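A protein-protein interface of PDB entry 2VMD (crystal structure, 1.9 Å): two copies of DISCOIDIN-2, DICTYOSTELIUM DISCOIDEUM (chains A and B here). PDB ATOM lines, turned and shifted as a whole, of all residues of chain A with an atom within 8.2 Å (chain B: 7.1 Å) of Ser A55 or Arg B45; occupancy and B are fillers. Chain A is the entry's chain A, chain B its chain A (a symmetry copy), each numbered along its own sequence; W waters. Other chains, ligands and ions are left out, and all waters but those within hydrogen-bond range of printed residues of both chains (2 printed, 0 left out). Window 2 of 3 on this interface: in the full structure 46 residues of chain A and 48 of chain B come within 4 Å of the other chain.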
ATOM      1  N   SER A  20     -10.425 -18.118  -3.571  1.00  0.00           N
ATOM      2  CA  SER A  20     -10.151 -18.118  -5.013  1.00  0.00           C
ATOM      3  C   SER A  20      -8.663 -18.192  -5.298  1.00  0.00           C
ATOM      4  O   SER A  20      -7.828 -17.810  -4.458  1.00  0.00           O
ATOM      5  CB  SER A  20     -10.690 -16.855  -5.681  1.00  0.00           C
ATOM      6  OG  SER A  20     -10.163 -15.694  -5.041  1.00  0.00           O
ATOM      7  N   SER A  21      -8.352 -18.721  -6.482  1.00  0.00           N
ATOM      8  CA  SER A  21      -6.981 -18.732  -7.032  1.00  0.00           C
ATOM      9  C   SER A  21      -6.461 -17.302  -7.238  1.00  0.00           C
ATOM     10  O   SER A  21      -5.435 -16.916  -6.685  1.00  0.00           O
ATOM     11  CB  SER A  21      -7.015 -19.477  -8.381  1.00  0.00           C
ATOM     12  OG  SER A  21      -8.155 -19.007  -9.116  1.00  0.00           O
ATOM     13  N   THR A  22      -7.199 -16.498  -8.010  1.00  0.00           N
ATOM     14  CA  THR A  22      -6.909 -15.057  -8.174  1.00  0.00           C
ATOM     15  C   THR A  22      -8.249 -14.281  -8.197  1.00  0.00           C
ATOM     16  O   THR A  22      -9.301 -14.877  -8.436  1.00  0.00           O
ATOM     17  CB  THR A  22      -6.073 -14.736  -9.461  1.00  0.00           C
ATOM     18  OG1 THR A  22      -6.852 -15.069 -10.645  1.00  0.00           O
ATOM     19  CG2 THR A  22      -4.797 -15.540  -9.498  1.00  0.00           C
ATOM     20  N   ASP A  23      -8.187 -12.964  -7.936  1.00  0.00           N
ATOM     21  CA  ASP A  23      -9.324 -12.060  -8.058  1.00  0.00           C
ATOM     22  C   ASP A  23      -8.877 -10.938  -8.973  1.00  0.00           C
ATOM     23  O   ASP A  23      -7.752 -10.466  -8.842  1.00  0.00           O
ATOM     24  CB  ASP A  23      -9.682 -11.385  -6.725  1.00  0.00           C
ATOM     25  CG  ASP A  23     -10.209 -12.341  -5.692  1.00  0.00           C
ATOM     26  OD1 ASP A  23     -10.752 -13.424  -6.053  1.00  0.00           O
ATOM     27  OD2 ASP A  23     -10.102 -11.972  -4.501  1.00  0.00           O
ATOM     28  N   TYR A  24      -9.772 -10.460  -9.831  1.00  0.00           N
ATOM     29  CA  TYR A  24      -9.479  -9.276 -10.661  1.00  0.00           C
ATOM     30  C   TYR A  24      -8.992  -8.121  -9.812  1.00  0.00           C
ATOM     31  O   TYR A  24      -7.987  -7.483 -10.117  1.00  0.00           O
ATOM     32  CB  TYR A  24     -10.684  -8.870 -11.467  1.00  0.00           C
ATOM     33  CG  TYR A  24     -10.359  -7.936 -12.601  1.00  0.00           C
ATOM     34  CD1 TYR A  24      -9.799  -8.428 -13.799  1.00  0.00           C
ATOM     35  CD2 TYR A  24     -10.626  -6.571 -12.499  1.00  0.00           C
ATOM     36  CE1 TYR A  24      -9.516  -7.565 -14.861  1.00  0.00           C
ATOM     37  CE2 TYR A  24     -10.343  -5.696 -13.557  1.00  0.00           C
ATOM     38  CZ  TYR A  24      -9.791  -6.211 -14.722  1.00  0.00           C
ATOM     39  OH  TYR A  24      -9.531  -5.374 -15.763  1.00  0.00           O
ATOM     40  N   ASN A  25      -9.694  -7.922  -8.696  1.00  0.00           N
ATOM     41  CA  ASN A  25      -9.203  -7.177  -7.524  1.00  0.00           C
ATOM     42  C   ASN A  25     -10.197  -7.479  -6.386  1.00  0.00           C
ATOM     43  O   ASN A  25     -11.125  -8.267  -6.582  1.00  0.00           O
ATOM     44  CB  ASN A  25      -9.085  -5.670  -7.826  1.00  0.00           C
ATOM     45  CG  ASN A  25     -10.364  -5.090  -8.399  1.00  0.00           C
ATOM     46  OD1 ASN A  25     -11.438  -5.363  -7.902  1.00  0.00           O
ATOM     47  ND2 ASN A  25     -10.252  -4.326  -9.495  1.00  0.00           N
ATOM     48  N   ALA A  26     -10.087  -6.800  -5.239  1.00  0.00           N
ATOM     49  CA  ALA A  26     -10.901  -7.185  -4.079  1.00  0.00           C
ATOM     50  C   ALA A  26     -12.369  -6.890  -4.358  1.00  0.00           C
ATOM     51  O   ALA A  26     -13.254  -7.482  -3.752  1.00  0.00           O
ATOM     52  CB  ALA A  26     -10.463  -6.404  -2.847  1.00  0.00           C
ATOM     53  N   HIS A  28     -13.795  -7.652  -6.924  1.00  0.00           N
ATOM     54  CA  HIS A  28     -14.296  -8.821  -7.687  1.00  0.00           C
ATOM     55  C   HIS A  28     -14.086 -10.163  -6.919  1.00  0.00           C
ATOM     56  O   HIS A  28     -13.955 -11.237  -7.517  1.00  0.00           O
ATOM     57  CB  HIS A  28     -13.610  -8.892  -9.069  1.00  0.00           C
ATOM     58  CG  HIS A  28     -13.816  -7.677  -9.929  1.00  0.00           C
ATOM     59  ND1 HIS A  28     -13.222  -6.456  -9.664  1.00  0.00           N
ATOM     60  CD2 HIS A  28     -14.558  -7.495 -11.050  1.00  0.00           C
ATOM     61  CE1 HIS A  28     -13.588  -5.575 -10.583  1.00  0.00           C
ATOM     62  NE2 HIS A  28     -14.380  -6.188 -11.450  1.00  0.00           N
ATOM     63  N   TRP A  52     -17.757 -13.278  -8.294  1.00  0.00           N
ATOM     64  CA  TRP A  52     -16.321 -13.401  -8.273  1.00  0.00           C
ATOM     65  C   TRP A  52     -15.825 -13.316  -9.734  1.00  0.00           C
ATOM     66  O   TRP A  52     -16.440 -13.921 -10.631  1.00  0.00           O
ATOM     67  CB  TRP A  52     -15.905 -14.763  -7.728  1.00  0.00           C
ATOM     68  CG  TRP A  52     -14.428 -15.081  -7.997  1.00  0.00           C
ATOM     69  CD1 TRP A  52     -13.342 -14.449  -7.469  1.00  0.00           C
ATOM     70  CD2 TRP A  52     -13.916 -16.139  -8.841  1.00  0.00           C
ATOM     71  NE1 TRP A  52     -12.174 -15.030  -7.969  1.00  0.00           N
ATOM     72  CE2 TRP A  52     -12.508 -16.079  -8.787  1.00  0.00           C
ATOM     73  CE3 TRP A  52     -14.524 -17.123  -9.638  1.00  0.00           C
ATOM     74  CZ2 TRP A  52     -11.681 -16.976  -9.495  1.00  0.00           C
ATOM     75  CZ3 TRP A  52     -13.688 -18.023 -10.366  1.00  0.00           C
ATOM     76  CH2 TRP A  52     -12.297 -17.948 -10.264  1.00  0.00           C
ATOM     77  N   SER A  53     -14.712 -12.609  -9.961  1.00  0.00           N
ATOM     78  CA  SER A  53     -14.039 -12.614 -11.275  1.00  0.00           C
ATOM     79  C   SER A  53     -12.574 -12.868 -11.020  1.00  0.00           C
ATOM     80  O   SER A  53     -11.975 -12.288 -10.102  1.00  0.00           O
ATOM     81  CB  SER A  53     -14.220 -11.296 -12.035  1.00  0.00           C
ATOM     82  OG  SER A  53     -15.605 -10.986 -12.160  1.00  0.00           O
ATOM     83  N   SER A  54     -11.997 -13.760 -11.804  1.00  0.00           N
ATOM     84  CA  SER A  54     -10.577 -14.042 -11.650  1.00  0.00           C
ATOM     85  C   SER A  54      -9.742 -12.901 -12.163  1.00  0.00           C
ATOM     86  O   SER A  54     -10.240 -11.978 -12.836  1.00  0.00           O
ATOM     87  CB  SER A  54     -10.192 -15.331 -12.407  1.00  0.00           C
ATOM     88  OG  SER A  54     -10.057 -15.040 -13.790  1.00  0.00           O
ATOM     89  N   SER A  55      -8.444 -12.948 -11.886  1.00  0.00           N
ATOM     90  CA  SER A  55      -7.521 -11.982 -12.504  1.00  0.00           C
ATOM     91  C   SER A  55      -6.853 -12.644 -13.703  1.00  0.00           C
ATOM     92  O   SER A  55      -6.812 -12.089 -14.786  1.00  0.00           O
ATOM     93  CB  SER A  55      -6.424 -11.547 -11.537  1.00  0.00           C
ATOM     94  OG  SER A  55      -5.605 -10.553 -12.162  1.00  0.00           O
ATOM     95  N   VAL A  56      -6.329 -13.843 -13.500  1.00  0.00           N
ATOM     96  CA  VAL A  56      -5.687 -14.568 -14.595  1.00  0.00           C
ATOM     97  C   VAL A  56      -6.776 -15.259 -15.401  1.00  0.00           C
ATOM     98  O   VAL A  56      -7.708 -15.851 -14.812  1.00  0.00           O
ATOM     99  CB  VAL A  56      -4.608 -15.530 -14.041  1.00  0.00           C
ATOM    100  CG1 VAL A  56      -3.971 -16.449 -15.150  1.00  0.00           C
ATOM    101  CG2 VAL A  56      -3.507 -14.760 -13.328  1.00  0.00           C
ATOM    102  N   LEU A  57      -6.713 -15.161 -16.734  1.00  0.00           N
ATOM    103  CA  LEU A  57      -7.624 -15.932 -17.571  1.00  0.00           C
ATOM    104  C   LEU A  57      -6.911 -17.134 -18.143  1.00  0.00           C
ATOM    105  O   LEU A  57      -6.180 -17.023 -19.111  1.00  0.00           O
ATOM    106  CB  LEU A  57      -8.292 -15.114 -18.710  1.00  0.00           C
ATOM    107  CG  LEU A  57      -9.174 -13.911 -18.335  1.00  0.00           C
ATOM    108  CD1 LEU A  57      -9.598 -13.158 -19.588  1.00  0.00           C
ATOM    109  CD2 LEU A  57     -10.367 -14.310 -17.576  1.00  0.00           C
ATOM    110  N   ASP A  58      -7.120 -18.278 -17.523  1.00  0.00           N
ATOM    111  CA  ASP A  58      -6.565 -19.536 -18.016  1.00  0.00           C
ATOM    112  C   ASP A  58      -7.449 -20.678 -17.514  1.00  0.00           C
ATOM    113  O   ASP A  58      -8.546 -20.416 -17.049  1.00  0.00           O
ATOM    114  CB  ASP A  58      -5.079 -19.703 -17.685  1.00  0.00           C
ATOM    115  CG  ASP A  58      -4.816 -19.884 -16.228  1.00  0.00           C
ATOM    116  OD1 ASP A  58      -5.750 -19.938 -15.410  1.00  0.00           O
ATOM    117  OD2 ASP A  58      -3.634 -19.937 -15.893  1.00  0.00           O
ATOM    118  N   GLN A  61      -7.911 -21.623 -12.813  1.00  0.00           N
ATOM    119  CA  GLN A  61      -8.520 -20.776 -11.779  1.00  0.00           C
ATOM    120  C   GLN A  61      -9.616 -21.568 -11.065  1.00  0.00           C
ATOM    121  O   GLN A  61     -10.135 -22.545 -11.619  1.00  0.00           O
ATOM    122  CB  GLN A  61      -9.100 -19.506 -12.406  1.00  0.00           C
ATOM    123  CG  GLN A  61      -8.107 -18.732 -13.254  1.00  0.00           C
ATOM    124  CD  GLN A  61      -6.923 -18.301 -12.429  1.00  0.00           C
ATOM    125  OE1 GLN A  61      -7.074 -17.650 -11.396  1.00  0.00           O
ATOM    126  NE2 GLN A  61      -5.745 -18.706 -12.847  1.00  0.00           N
ATOM    127  N   HIS A 144     -14.983 -13.215 -19.429  1.00  0.00           N
ATOM    128  CA  HIS A 144     -14.124 -13.321 -18.262  1.00  0.00           C
ATOM    129  C   HIS A 144     -14.612 -14.508 -17.442  1.00  0.00           C
ATOM    130  O   HIS A 144     -15.800 -14.892 -17.518  1.00  0.00           O
ATOM    131  CB  HIS A 144     -14.154 -12.021 -17.440  1.00  0.00           C
ATOM    132  CG  HIS A 144     -12.936 -11.809 -16.586  1.00  0.00           C
ATOM    133  ND1 HIS A 144     -11.905 -10.973 -16.956  1.00  0.00           N
ATOM    134  CD2 HIS A 144     -12.589 -12.324 -15.383  1.00  0.00           C
ATOM    135  CE1 HIS A 144     -10.968 -10.997 -16.020  1.00  0.00           C
ATOM    136  NE2 HIS A 144     -11.357 -11.820 -15.061  1.00  0.00           N
ATOM    137  N   ILE A 145     -13.703 -15.062 -16.649  1.00  0.00           N
ATOM    138  CA  ILE A 145     -14.035 -16.062 -15.640  1.00  0.00           C
ATOM    139  C   ILE A 145     -14.768 -15.307 -14.522  1.00  0.00           C
ATOM    140  O   ILE A 145     -14.131 -14.745 -13.658  1.00  0.00           O
ATOM    141  CB  ILE A 145     -12.754 -16.782 -15.104  1.00  0.00           C
ATOM    142  CG1 ILE A 145     -12.062 -17.551 -16.253  1.00  0.00           C
ATOM    143  CG2 ILE A 145     -13.119 -17.728 -13.919  1.00  0.00           C
ATOM    144  CD1 ILE A 145     -10.684 -18.078 -15.917  1.00  0.00           C
ATOM    145  N   ASN B  39      -0.668 -13.724  -8.755  1.00  0.00           N
ATOM    146  CA  ASN B  39      -1.782 -13.333  -9.597  1.00  0.00           C
ATOM    147  C   ASN B  39      -1.253 -12.848 -10.944  1.00  0.00           C
ATOM    148  O   ASN B  39      -0.220 -13.350 -11.411  1.00  0.00           O
ATOM    149  CB  ASN B  39      -2.725 -12.360  -8.861  1.00  0.00           C
ATOM    150  CG  ASN B  39      -2.019 -11.139  -8.301  1.00  0.00           C
ATOM    151  OD1 ASN B  39      -0.967 -10.743  -8.792  1.00  0.00           O
ATOM    152  ND2 ASN B  39      -2.641 -10.482  -7.308  1.00  0.00           N
ATOM    153  N   SER B  40      -1.926 -11.898 -11.567  1.00  0.00           N
ATOM    154  CA  SER B  40      -1.537 -11.513 -12.909  1.00  0.00           C
ATOM    155  C   SER B  40      -0.206 -10.775 -12.902  1.00  0.00           C
ATOM    156  O   SER B  40       0.011  -9.889 -12.096  1.00  0.00           O
ATOM    157  CB  SER B  40      -2.600 -10.646 -13.548  1.00  0.00           C
ATOM    158  OG  SER B  40      -2.228 -10.377 -14.870  1.00  0.00           O
ATOM    159  N   LYS B  41       0.671 -11.146 -13.826  1.00  0.00           N
ATOM    160  CA  LYS B  41       1.997 -10.517 -13.910  1.00  0.00           C
ATOM    161  C   LYS B  41       1.970  -9.227 -14.727  1.00  0.00           C
ATOM    162  O   LYS B  41       3.012  -8.638 -15.021  1.00  0.00           O
ATOM    163  CB  LYS B  41       3.000 -11.510 -14.495  1.00  0.00           C
ATOM    164  CG  LYS B  41       3.279 -12.661 -13.574  1.00  0.00           C
ATOM    165  CD  LYS B  41       3.727 -12.140 -12.223  1.00  0.00           C
ATOM    166  CE  LYS B  41       4.112 -13.272 -11.295  1.00  0.00           C
ATOM    167  NZ  LYS B  41       2.929 -13.760 -10.552  1.00  0.00           N
ATOM    168  N   ASP B  42       0.765  -8.800 -15.080  1.00  0.00           N
ATOM    169  CA  ASP B  42       0.509  -7.555 -15.786  1.00  0.00           C
ATOM    170  C   ASP B  42       0.927  -6.319 -14.978  1.00  0.00           C
ATOM    171  O   ASP B  42       0.360  -6.036 -13.928  1.00  0.00           O
ATOM    172  CB  ASP B  42      -0.991  -7.488 -16.119  1.00  0.00           C
ATOM    173  CG  ASP B  42      -1.379  -6.227 -16.858  1.00  0.00           C
ATOM    174  OD1 ASP B  42      -0.514  -5.334 -16.989  1.00  0.00           O
ATOM    175  OD2 ASP B  42      -2.554  -6.135 -17.319  1.00  0.00           O
ATOM    176  N   ALA B  43       1.894  -5.558 -15.494  1.00  0.00           N
ATOM    177  CA  ALA B  43       2.406  -4.369 -14.794  1.00  0.00           C
ATOM    178  C   ALA B  43       1.504  -3.147 -14.942  1.00  0.00           C
ATOM    179  O   ALA B  43       1.701  -2.129 -14.274  1.00  0.00           O
ATOM    180  CB  ALA B  43       3.813  -4.052 -15.265  1.00  0.00           C
ATOM    181  N   SER B  44       0.497  -3.237 -15.798  1.00  0.00           N
ATOM    182  CA  SER B  44      -0.320  -2.063 -16.084  1.00  0.00           C
ATOM    183  C   SER B  44      -1.589  -1.947 -15.240  1.00  0.00           C
ATOM    184  O   SER B  44      -2.246  -0.893 -15.252  1.00  0.00           O
ATOM    185  CB  SER B  44      -0.680  -2.029 -17.568  1.00  0.00           C
ATOM    186  OG  SER B  44      -1.805  -2.841 -17.830  1.00  0.00           O
ATOM    187  N   ARG B  45      -1.930  -3.024 -14.523  1.00  0.00           N
ATOM    188  CA  ARG B  45      -3.143  -3.073 -13.688  1.00  0.00           C
ATOM    189  C   ARG B  45      -2.823  -3.768 -12.373  1.00  0.00           C
ATOM    190  O   ARG B  45      -2.237  -4.843 -12.365  1.00  0.00           O
ATOM    191  CB  ARG B  45      -4.226  -3.881 -14.399  1.00  0.00           C
ATOM    192  CG  ARG B  45      -5.591  -3.783 -13.811  1.00  0.00           C
ATOM    193  CD  ARG B  45      -6.563  -4.629 -14.611  1.00  0.00           C
ATOM    194  NE  ARG B  45      -6.169  -6.044 -14.709  1.00  0.00           N
ATOM    195  CZ  ARG B  45      -6.343  -6.955 -13.745  1.00  0.00           C
ATOM    196  NH1 ARG B  45      -6.861  -6.593 -12.582  1.00  0.00           N
ATOM    197  NH2 ARG B  45      -5.984  -8.221 -13.945  1.00  0.00           N
ATOM    198  N   PHE B  46      -3.222  -3.164 -11.266  1.00  0.00           N
ATOM    199  CA  PHE B  46      -3.028  -3.779  -9.972  1.00  0.00           C
ATOM    200  C   PHE B  46      -4.217  -4.653  -9.591  1.00  0.00           C
ATOM    201  O   PHE B  46      -5.325  -4.144  -9.428  1.00  0.00           O
ATOM    202  CB  PHE B  46      -2.858  -2.701  -8.930  1.00  0.00           C
ATOM    203  CG  PHE B  46      -2.414  -3.209  -7.614  1.00  0.00           C
ATOM    204  CD1 PHE B  46      -1.277  -4.006  -7.506  1.00  0.00           C
ATOM    205  CD2 PHE B  46      -3.129  -2.890  -6.467  1.00  0.00           C
ATOM    206  CE1 PHE B  46      -0.853  -4.475  -6.268  1.00  0.00           C
ATOM    207  CE2 PHE B  46      -2.708  -3.351  -5.232  1.00  0.00           C
ATOM    208  CZ  PHE B  46      -1.572  -4.142  -5.131  1.00  0.00           C
ATOM    209  N   ASP B  47      -3.965  -5.958  -9.467  1.00  0.00           N
ATOM    210  CA  ASP B  47      -4.965  -6.933  -9.014  1.00  0.00           C
ATOM    211  C   ASP B  47      -4.808  -7.344  -7.537  1.00  0.00           C
ATOM    212  O   ASP B  47      -5.473  -8.276  -7.074  1.00  0.00           O
ATOM    213  CB  ASP B  47      -4.994  -8.176  -9.922  1.00  0.00           C
ATOM    214  CG  ASP B  47      -3.640  -8.820 -10.084  1.00  0.00           C
ATOM    215  OD1 ASP B  47      -2.620  -8.287  -9.604  1.00  0.00           O
ATOM    216  OD2 ASP B  47      -3.578  -9.900 -10.694  1.00  0.00           O
ATOM    217  N   GLY B  48      -3.951  -6.639  -6.797  1.00  0.00           N
ATOM    218  CA  GLY B  48      -3.743  -6.934  -5.396  1.00  0.00           C
ATOM    219  C   GLY B  48      -2.320  -7.381  -5.116  1.00  0.00           C
ATOM    220  O   GLY B  48      -1.640  -7.923  -5.993  1.00  0.00           O
HETATM  221  O   HOH W   1      -5.634 -11.394  -7.134  1.00  0.00           O
HETATM  222  O   HOH W   2      -7.701  -4.025 -11.238  1.00  0.00           O
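The backbone carbonyl oxygen of Tyr A24 lies within hydrogen-bond range of the guanidinium group of Arg B45, at 2.9 Å. The side-chain hydroxyl of Ser A55 sits at hydrogen-bond distance from the guanidinium group of Arg B45, at 3.0 Å. The side-chain carboxylate of Asp B47 is in hydrogen-bond range of the side-chain hydroxyl of Ser A55 (2.6 Å).
OG of Ser A20 is in hydrogen-bond range of OD1 of Asp A23. NE1 of Trp A52 lies within hydrogen-bond range of O of Thr A22, at 2.9 Å. OE1 of Gln A61 lies within hydrogen-bond range of OG1 of Thr A22, at 2.7 Å. The backbone NH (N) of Tyr A24 lies close to the backbone carbonyl oxygen (O) of Ser A54 (3.4 Å). The backbone carbonyl oxygen (O) of Asn B39 is in hydrogen-bond range of the side-chain amino group (NZ) of Lys B41 (3.3 Å). OG of Ser B40 sits close to N of Asp B42.
Among the printed residues, merely in contact across the chains: Thr A22 with Asn B39 (3.7 Å), Asp A23 with Asp B47 (3.6 Å), Tyr A24 with Asp B47 (3.1 Å), Asn A25 with Asp B47 (3.9 Å), Ser A55 with Ser B40 (3.3 Å), Val A56 with Asn B39 (3.8 Å) and Val A56 with Ser B40 (3.7 Å).
Ser A55 touches just these residues of chain B: Ser B40 (3.3 Å), Arg B45 (3.0 Å) and Asp B47 (2.6 Å). Arg B45 touches just these residues of chain A: Tyr A24 and Ser A55. No residue of chain A comes within 4 Å of Ser B44. Printed residues of chain A within 4 Å of Asn B39: Thr A22 (3.7 Å) and Val A56 (3.8 Å). Of the printed residues of chain B, Val A56 touches Asn B39 and Ser B40. Printed residues of chain A within 4 Å of Asp B47: Asp A23, Tyr A24, Asn A25 and Ser A55. Ile A145 touches none of the printed residues of chain B. Asp A58 touches none of the printed residues of chain B.
Hydrophobic or aromatic side chains of chain A within 4 Å of the printed part of chain B: Tyr A24 and Val A56. Along chain A the printed residues that touch a printed residue of chain B span positions 22 to 56. Of the 10 printed residues of chain B, 4 touch a printed residue of chain A. Along chain B the printed residues that touch a printed residue of chain A span positions 39 to 47. Among the printed residues, 10 pairs touch across the chains.
No position is printed for both chains. Of the 10 pairs that touch across the chains among the printed residues, none has its exchanged pair printed and touching as well.
Water W1 lies within hydrogen-bond range of O of Asp A23, O of Asp B47 and ND2 of Asn B39. Water W2 lies within hydrogen-bond range of O of Phe B46 (3.0 Å), NH1 of Arg B45 (3.0 Å) and ND2 of Asn A25 (3.1 Å).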
